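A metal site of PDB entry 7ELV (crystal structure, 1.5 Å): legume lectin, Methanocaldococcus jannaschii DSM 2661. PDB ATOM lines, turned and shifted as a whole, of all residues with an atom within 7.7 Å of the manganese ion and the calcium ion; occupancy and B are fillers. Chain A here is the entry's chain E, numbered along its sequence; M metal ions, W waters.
The backbone carbonyl oxygen (O) of Thr 110 lies within hydrogen-bond range of a ring nitrogen (ND1) of His 112. The backbone carbonyl oxygen (O) of Phe 104 sits at hydrogen-bond distance from the backbone NH (N) of His 123 (3.2 Å). The side-chain carboxylate (OE1) of Glu 96 lies close to the side-chain carboxylate (OD2) of Asp 116 (2.5 Å). O of Ala 114 is in hydrogen-bond range of N of Glu 96 (2.8 Å).
The nearest printed residue that does not touch the manganese ion is Ile 121 (4.4 Å).
The nearest printed residue that does not touch the calcium ion is Phe 104 (4.5 Å).
The manganese ion is bound by the side-chain carboxylate of Glu 96 (2.1 Å), the side-chain carboxylate of Asp 98 (2.1 Å), the side-chain carboxylate of Asp 105 (2.2 Å), a ring nitrogen (NE2) of His 123 (2.2 Å), water W2 (2.3 Å) and a ring nitrogen (NE2) of His 112 (2.3 Å). The manganese ion has six donor atoms within binding distance.
O of Trp 100 is bound to the calcium ion. OD1 of Asn 102 is bound to the calcium ion, 2.4 Å away. OD2 of Asp 105 is bound to the calcium ion (2.4 Å). Water W1 binds the calcium ion, 2.4 Å away. Water W3 is bound to the calcium ion (2.4 Å). OD1 of Asp 98 binds the calcium ion, at 2.5 Å. The calcium ion is bound by OD2 of Asp 98.
Water W2 lies within hydrogen-bond range of OE1 of Glu 96 (2.7 Å) and O of Ile 121 (2.9 Å).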
ATOM      1  N   ALA A  62      28.786  -1.781 -11.931  1.00  0.00           N
ATOM      2  CA  ALA A  62      27.823  -1.428 -12.974  1.00  0.00           C
ATOM      3  C   ALA A  62      27.730  -2.576 -13.951  1.00  0.00           C
ATOM      4  O   ALA A  62      28.582  -3.470 -13.873  1.00  0.00           O
ATOM      5  CB  ALA A  62      28.262  -0.166 -13.672  1.00  0.00           C
ATOM      6  N   ASP A  63      26.743  -2.561 -14.866  1.00  0.00           N
ATOM      7  CA  ASP A  63      25.681  -1.580 -15.034  1.00  0.00           C
ATOM      8  C   ASP A  63      24.302  -2.168 -14.714  1.00  0.00           C
ATOM      9  O   ASP A  63      23.393  -1.355 -14.484  1.00  0.00           O
ATOM     10  CB  ASP A  63      25.630  -1.047 -16.466  1.00  0.00           C
ATOM     11  CG  ASP A  63      26.569   0.113 -16.668  1.00  0.00           C
ATOM     12  OD1 ASP A  63      26.117   1.229 -16.357  1.00  0.00           O
ATOM     13  OD2 ASP A  63      27.714  -0.127 -17.106  1.00  0.00           O
ATOM     14  N   GLY A  64      24.117  -3.484 -14.759  1.00  0.00           N
ATOM     15  CA  GLY A  64      22.816  -4.105 -14.562  1.00  0.00           C
ATOM     16  C   GLY A  64      22.410  -5.023 -15.699  1.00  0.00           C
ATOM     17  O   GLY A  64      23.173  -5.302 -16.633  1.00  0.00           O
ATOM     18  N   GLY A  81      27.392  -0.799 -21.358  1.00  0.00           N
ATOM     19  CA  GLY A  81      27.312   0.213 -20.295  1.00  0.00           C
ATOM     20  C   GLY A  81      25.870   0.386 -19.794  1.00  0.00           C
ATOM     21  O   GLY A  81      25.154  -0.642 -19.541  1.00  0.00           O
ATOM     22  N   GLY A  82      25.405   1.630 -19.693  1.00  0.00           N
ATOM     23  CA  GLY A  82      24.083   1.935 -19.126  1.00  0.00           C
ATOM     24  C   GLY A  82      22.960   1.469 -20.040  1.00  0.00           C
ATOM     25  O   GLY A  82      21.815   1.538 -19.651  1.00  0.00           O
ATOM     26  N   ASP A  83      23.252   1.009 -21.248  1.00  0.00           N
ATOM     27  CA  ASP A  83      22.238   0.368 -22.112  1.00  0.00           C
ATOM     28  C   ASP A  83      21.906  -1.057 -21.614  1.00  0.00           C
ATOM     29  O   ASP A  83      20.922  -1.595 -22.075  1.00  0.00           O
ATOM     30  CB  ASP A  83      22.707   0.317 -23.557  1.00  0.00           C
ATOM     31  CG  ASP A  83      22.363   1.558 -24.371  1.00  0.00           C
ATOM     32  OD1 ASP A  83      21.665   2.443 -23.853  1.00  0.00           O
ATOM     33  OD2 ASP A  83      22.711   1.580 -25.536  1.00  0.00           O
ATOM     34  N   LEU A  84      22.720  -1.635 -20.741  1.00  0.00           N
ATOM     35  CA  LEU A  84      22.433  -2.925 -20.048  1.00  0.00           C
ATOM     36  C   LEU A  84      22.369  -4.105 -21.014  1.00  0.00           C
ATOM     37  O   LEU A  84      21.809  -5.118 -20.630  1.00  0.00           O
ATOM     38  CB  LEU A  84      21.081  -2.825 -19.303  1.00  0.00           C
ATOM     39  CG  LEU A  84      20.871  -1.603 -18.408  1.00  0.00           C
ATOM     40  CD1 LEU A  84      19.544  -1.692 -17.632  1.00  0.00           C
ATOM     41  CD2 LEU A  84      22.024  -1.456 -17.466  1.00  0.00           C
ATOM     42  N   GLU A  96      14.326  -3.985 -16.013  1.00  0.00           N
ATOM     43  CA  GLU A  96      15.752  -3.795 -15.735  1.00  0.00           C
ATOM     44  C   GLU A  96      16.003  -3.901 -14.243  1.00  0.00           C
ATOM     45  O   GLU A  96      15.145  -3.421 -13.471  1.00  0.00           O
ATOM     46  CB  GLU A  96      16.298  -2.462 -16.281  1.00  0.00           C
ATOM     47  CG  GLU A  96      15.629  -1.219 -15.752  1.00  0.00           C
ATOM     48  CD  GLU A  96      16.370   0.063 -16.137  1.00  0.00           C
ATOM     49  OE1 GLU A  96      16.581   0.320 -17.358  1.00  0.00           O
ATOM     50  OE2 GLU A  96      16.781   0.771 -15.166  1.00  0.00           O
ATOM     51  N   VAL A  97      17.172  -4.390 -13.893  1.00  0.00           N
ATOM     52  CA  VAL A  97      17.756  -4.291 -12.535  1.00  0.00           C
ATOM     53  C   VAL A  97      19.046  -3.525 -12.763  1.00  0.00           C
ATOM     54  O   VAL A  97      20.022  -4.062 -13.299  1.00  0.00           O
ATOM     55  CB  VAL A  97      17.968  -5.641 -11.861  1.00  0.00           C
ATOM     56  CG1 VAL A  97      18.520  -5.371 -10.480  1.00  0.00           C
ATOM     57  CG2 VAL A  97      16.647  -6.402 -11.778  1.00  0.00           C
ATOM     58  N   ASP A  98      19.014  -2.237 -12.419  1.00  0.00           N
ATOM     59  CA  ASP A  98      19.985  -1.228 -12.864  1.00  0.00           C
ATOM     60  C   ASP A  98      20.866  -0.894 -11.672  1.00  0.00           C
ATOM     61  O   ASP A  98      20.315  -0.445 -10.658  1.00  0.00           O
ATOM     62  CB  ASP A  98      19.259  -0.025 -13.434  1.00  0.00           C
ATOM     63  CG  ASP A  98      20.163   1.079 -13.968  1.00  0.00           C
ATOM     64  OD1 ASP A  98      21.361   1.034 -13.667  1.00  0.00           O
ATOM     65  OD2 ASP A  98      19.651   1.916 -14.693  1.00  0.00           O
ATOM     66  N   THR A  99      22.186  -1.048 -11.779  1.00  0.00           N
ATOM     67  CA  THR A  99      23.101  -0.969 -10.617  1.00  0.00           C
ATOM     68  C   THR A  99      24.044   0.241 -10.754  1.00  0.00           C
ATOM     69  O   THR A  99      24.981   0.307  -9.964  1.00  0.00           O
ATOM     70  CB  THR A  99      23.870  -2.282 -10.436  1.00  0.00           C
ATOM     71  OG1 THR A  99      24.613  -2.488 -11.630  1.00  0.00           O
ATOM     72  CG2 THR A  99      22.945  -3.452 -10.155  1.00  0.00           C
ATOM     73  N   TRP A 100      23.786   1.172 -11.660  1.00  0.00           N
ATOM     74  CA  TRP A 100      24.650   2.366 -11.804  1.00  0.00           C
ATOM     75  C   TRP A 100      23.777   3.532 -12.188  1.00  0.00           C
ATOM     76  O   TRP A 100      23.018   3.488 -13.142  1.00  0.00           O
ATOM     77  CB  TRP A 100      25.754   2.115 -12.831  1.00  0.00           C
ATOM     78  CG  TRP A 100      26.543   3.348 -13.139  1.00  0.00           C
ATOM     79  CD1 TRP A 100      26.243   4.344 -14.033  1.00  0.00           C
ATOM     80  CD2 TRP A 100      27.788   3.676 -12.536  1.00  0.00           C
ATOM     81  NE1 TRP A 100      27.244   5.272 -14.026  1.00  0.00           N
ATOM     82  CE2 TRP A 100      28.181   4.893 -13.121  1.00  0.00           C
ATOM     83  CE3 TRP A 100      28.578   3.071 -11.572  1.00  0.00           C
ATOM     84  CZ2 TRP A 100      29.393   5.505 -12.777  1.00  0.00           C
ATOM     85  CZ3 TRP A 100      29.769   3.677 -11.228  1.00  0.00           C
ATOM     86  CH2 TRP A 100      30.159   4.875 -11.823  1.00  0.00           C
ATOM     87  N   LEU A 101      23.843   4.623 -11.404  1.00  0.00           N
ATOM     88  CA  LEU A 101      22.959   5.771 -11.668  1.00  0.00           C
ATOM     89  C   LEU A 101      23.543   6.643 -12.758  1.00  0.00           C
ATOM     90  O   LEU A 101      24.515   7.399 -12.492  1.00  0.00           O
ATOM     91  CB  LEU A 101      22.806   6.582 -10.374  1.00  0.00           C
ATOM     92  CG  LEU A 101      21.918   6.004  -9.313  1.00  0.00           C
ATOM     93  CD1 LEU A 101      21.976   6.858  -8.057  1.00  0.00           C
ATOM     94  CD2 LEU A 101      20.457   5.923  -9.780  1.00  0.00           C
ATOM     95  N   ASN A 102      22.931   6.596 -13.923  1.00  0.00           N
ATOM     96  CA  ASN A 102      23.222   7.498 -15.054  1.00  0.00           C
ATOM     97  C   ASN A 102      22.420   8.791 -14.915  1.00  0.00           C
ATOM     98  O   ASN A 102      21.406   8.790 -14.237  1.00  0.00           O
ATOM     99  CB  ASN A 102      22.945   6.807 -16.386  1.00  0.00           C
ATOM    100  CG  ASN A 102      23.783   5.563 -16.586  1.00  0.00           C
ATOM    101  OD1 ASN A 102      23.370   4.466 -16.178  1.00  0.00           O
ATOM    102  ND2 ASN A 102      24.986   5.702 -17.141  1.00  0.00           N
ATOM    103  N   ASP A 103      22.776   9.865 -15.629  1.00  0.00           N
ATOM    104  CA  ASP A 103      21.942  11.096 -15.497  1.00  0.00           C
ATOM    105  C   ASP A 103      20.496  10.775 -15.934  1.00  0.00           C
ATOM    106  O   ASP A 103      19.538  11.272 -15.288  1.00  0.00           O
ATOM    107  CB  ASP A 103      22.550  12.273 -16.269  1.00  0.00           C
ATOM    108  CG  ASP A 103      23.119  11.909 -17.629  1.00  0.00           C
ATOM    109  OD1 ASP A 103      22.793  10.797 -18.140  1.00  0.00           O
ATOM    110  OD2 ASP A 103      23.879  12.748 -18.178  1.00  0.00           O
ATOM    111  N   PHE A 104      20.318   9.868 -16.901  1.00  0.00           N
ATOM    112  CA  PHE A 104      18.980   9.557 -17.465  1.00  0.00           C
ATOM    113  C   PHE A 104      18.166   8.634 -16.529  1.00  0.00           C
ATOM    114  O   PHE A 104      17.068   8.264 -16.906  1.00  0.00           O
ATOM    115  CB  PHE A 104      19.123   8.961 -18.877  1.00  0.00           C
ATOM    116  CG  PHE A 104      20.037   7.761 -18.997  1.00  0.00           C
ATOM    117  CD1 PHE A 104      19.653   6.540 -18.466  1.00  0.00           C
ATOM    118  CD2 PHE A 104      21.286   7.851 -19.602  1.00  0.00           C
ATOM    119  CE1 PHE A 104      20.471   5.425 -18.593  1.00  0.00           C
ATOM    120  CE2 PHE A 104      22.104   6.738 -19.705  1.00  0.00           C
ATOM    121  CZ  PHE A 104      21.681   5.521 -19.211  1.00  0.00           C
ATOM    122  N   ASP A 105      18.732   8.255 -15.399  1.00  0.00           N
ATOM    123  CA  ASP A 105      18.092   7.298 -14.472  1.00  0.00           C
ATOM    124  C   ASP A 105      17.152   8.027 -13.506  1.00  0.00           C
ATOM    125  O   ASP A 105      16.392   7.366 -12.811  1.00  0.00           O
ATOM    126  CB  ASP A 105      19.088   6.435 -13.719  1.00  0.00           C
ATOM    127  CG  ASP A 105      19.567   5.227 -14.502  1.00  0.00           C
ATOM    128  OD1 ASP A 105      18.667   4.622 -15.130  1.00  0.00           O
ATOM    129  OD2 ASP A 105      20.751   4.879 -14.396  1.00  0.00           O
ATOM    130  N   ALA A 106      17.174   9.357 -13.456  1.00  0.00           N
ATOM    131  CA  ALA A 106      16.250  10.078 -12.556  1.00  0.00           C
ATOM    132  C   ALA A 106      14.842   9.607 -12.879  1.00  0.00           C
ATOM    133  O   ALA A 106      14.488   9.447 -14.070  1.00  0.00           O
ATOM    134  CB  ALA A 106      16.395  11.565 -12.778  1.00  0.00           C
ATOM    135  N   ALA A 108      15.271   7.585 -10.119  1.00  0.00           N
ATOM    136  CA  ALA A 108      15.944   6.606  -9.272  1.00  0.00           C
ATOM    137  C   ALA A 108      17.059   7.267  -8.450  1.00  0.00           C
ATOM    138  O   ALA A 108      17.742   8.239  -8.931  1.00  0.00           O
ATOM    139  CB  ALA A 108      16.503   5.485 -10.134  1.00  0.00           C
ATOM    140  N   THR A 110      18.961   4.769  -6.136  1.00  0.00           N
ATOM    141  CA  THR A 110      19.807   3.644  -5.706  1.00  0.00           C
ATOM    142  C   THR A 110      19.814   2.641  -6.861  1.00  0.00           C
ATOM    143  O   THR A 110      19.157   2.908  -7.865  1.00  0.00           O
ATOM    144  CB  THR A 110      19.321   2.984  -4.418  1.00  0.00           C
ATOM    145  OG1 THR A 110      18.111   2.257  -4.671  1.00  0.00           O
ATOM    146  CG2 THR A 110      19.055   3.978  -3.306  1.00  0.00           C
ATOM    147  N   HIS A 112      18.056  -0.066  -8.858  1.00  0.00           N
ATOM    148  CA  HIS A 112      16.601   0.078  -9.034  1.00  0.00           C
ATOM    149  C   HIS A 112      16.062  -0.923 -10.034  1.00  0.00           C
ATOM    150  O   HIS A 112      16.837  -1.454 -10.852  1.00  0.00           O
ATOM    151  CB  HIS A 112      16.193   1.500  -9.449  1.00  0.00           C
ATOM    152  CG  HIS A 112      16.893   2.014 -10.671  1.00  0.00           C
ATOM    153  ND1 HIS A 112      18.149   2.591 -10.603  1.00  0.00           N
ATOM    154  CD2 HIS A 112      16.507   2.062 -11.980  1.00  0.00           C
ATOM    155  CE1 HIS A 112      18.500   2.943 -11.816  1.00  0.00           C
ATOM    156  NE2 HIS A 112      17.525   2.689 -12.667  1.00  0.00           N
ATOM    157  N   ILE A 113      14.784  -1.187  -9.913  1.00  0.00           N
ATOM    158  CA  ILE A 113      14.046  -2.002 -10.896  1.00  0.00           C
ATOM    159  C   ILE A 113      13.093  -1.099 -11.643  1.00  0.00           C
ATOM    160  O   ILE A 113      12.455  -0.205 -11.014  1.00  0.00           O
ATOM    161  CB  ILE A 113      13.483  -3.241 -10.152  1.00  0.00           C
ATOM    162  CG1 ILE A 113      12.965  -4.309 -11.115  1.00  0.00           C
ATOM    163  CG2 ILE A 113      12.453  -2.879  -9.116  1.00  0.00           C
ATOM    164  CD1 ILE A 113      12.913  -5.715 -10.526  1.00  0.00           C
ATOM    165  N   ALA A 114      12.940  -1.263 -12.951  1.00  0.00           N
ATOM    166  CA  ALA A 114      12.117  -0.391 -13.780  1.00  0.00           C
ATOM    167  C   ALA A 114      11.605  -1.145 -15.011  1.00  0.00           C
ATOM    168  O   ALA A 114      12.245  -2.144 -15.427  1.00  0.00           O
ATOM    169  CB  ALA A 114      12.875   0.849 -14.207  1.00  0.00           C
ATOM    170  N   ASP A 116      11.109  -0.696 -18.991  1.00  0.00           N
ATOM    171  CA  ASP A 116      11.547   0.053 -20.179  1.00  0.00           C
ATOM    172  C   ASP A 116      10.772  -0.418 -21.397  1.00  0.00           C
ATOM    173  O   ASP A 116      10.330  -1.561 -21.457  1.00  0.00           O
ATOM    174  CB  ASP A 116      13.020  -0.215 -20.423  1.00  0.00           C
ATOM    175  CG  ASP A 116      13.966   0.181 -19.326  1.00  0.00           C
ATOM    176  OD1 ASP A 116      13.623   1.121 -18.567  1.00  0.00           O
ATOM    177  OD2 ASP A 116      15.006  -0.466 -19.186  1.00  0.00           O
ATOM    178  N   ILE A 121      16.016   3.564 -22.242  1.00  0.00           N
ATOM    179  CA  ILE A 121      16.482   3.313 -20.852  1.00  0.00           C
ATOM    180  C   ILE A 121      16.366   4.607 -20.006  1.00  0.00           C
ATOM    181  O   ILE A 121      16.765   4.568 -18.837  1.00  0.00           O
ATOM    182  CB  ILE A 121      17.890   2.681 -20.821  1.00  0.00           C
ATOM    183  CG1 ILE A 121      18.934   3.354 -21.715  1.00  0.00           C
ATOM    184  CG2 ILE A 121      17.829   1.203 -21.201  1.00  0.00           C
ATOM    185  CD1 ILE A 121      19.116   4.796 -21.487  1.00  0.00           C
ATOM    186  N   ASN A 122      15.784   5.685 -20.561  1.00  0.00           N
ATOM    187  CA  ASN A 122      15.610   6.994 -19.869  1.00  0.00           C
ATOM    188  C   ASN A 122      14.255   7.011 -19.142  1.00  0.00           C
ATOM    189  O   ASN A 122      13.172   7.029 -19.830  1.00  0.00           O
ATOM    190  CB  ASN A 122      15.691   8.114 -20.900  1.00  0.00           C
ATOM    191  CG  ASN A 122      15.548   9.520 -20.349  1.00  0.00           C
ATOM    192  OD1 ASN A 122      14.674   9.788 -19.542  1.00  0.00           O
ATOM    193  ND2 ASN A 122      16.406  10.423 -20.816  1.00  0.00           N
ATOM    194  N   HIS A 123      14.269   7.033 -17.822  1.00  0.00           N
ATOM    195  CA  HIS A 123      12.989   6.769 -17.086  1.00  0.00           C
ATOM    196  C   HIS A 123      11.971   7.916 -17.258  1.00  0.00           C
ATOM    197  O   HIS A 123      10.767   7.628 -17.367  1.00  0.00           O
ATOM    198  CB  HIS A 123      13.286   6.385 -15.651  1.00  0.00           C
ATOM    199  CG  HIS A 123      14.160   5.165 -15.615  1.00  0.00           C
ATOM    200  ND1 HIS A 123      13.841   4.018 -16.361  1.00  0.00           N
ATOM    201  CD2 HIS A 123      15.284   4.900 -14.966  1.00  0.00           C
ATOM    202  CE1 HIS A 123      14.823   3.151 -16.137  1.00  0.00           C
ATOM    203  NE2 HIS A 123      15.691   3.638 -15.300  1.00  0.00           N
ATOM    204  N   PRO A 135      10.861   4.293 -11.629  1.00  0.00           N
ATOM    205  CA  PRO A 135      11.735   3.252 -11.127  1.00  0.00           C
ATOM    206  C   PRO A 135      11.519   3.050  -9.636  1.00  0.00           C
ATOM    207  O   PRO A 135      11.205   3.990  -8.889  1.00  0.00           O
ATOM    208  CB  PRO A 135      13.160   3.720 -11.409  1.00  0.00           C
ATOM    209  CG  PRO A 135      13.015   5.116 -11.950  1.00  0.00           C
ATOM    210  CD  PRO A 135      11.569   5.446 -12.181  1.00  0.00           C
HETATM  211 MN    MN M   1      17.674   2.707 -14.975  1.00  0.00          MN
HETATM  212 CA    CA M   2      21.903   2.938 -15.139  1.00  0.00          CA
HETATM  213  O   HOH W   1      23.558   1.277 -15.575  1.00  0.00           O
HETATM  214  O   HOH W   2      18.019   2.551 -17.257  1.00  0.00           O
HETATM  215  O   HOH W   3      20.866   2.417 -17.252  1.00  0.00           O
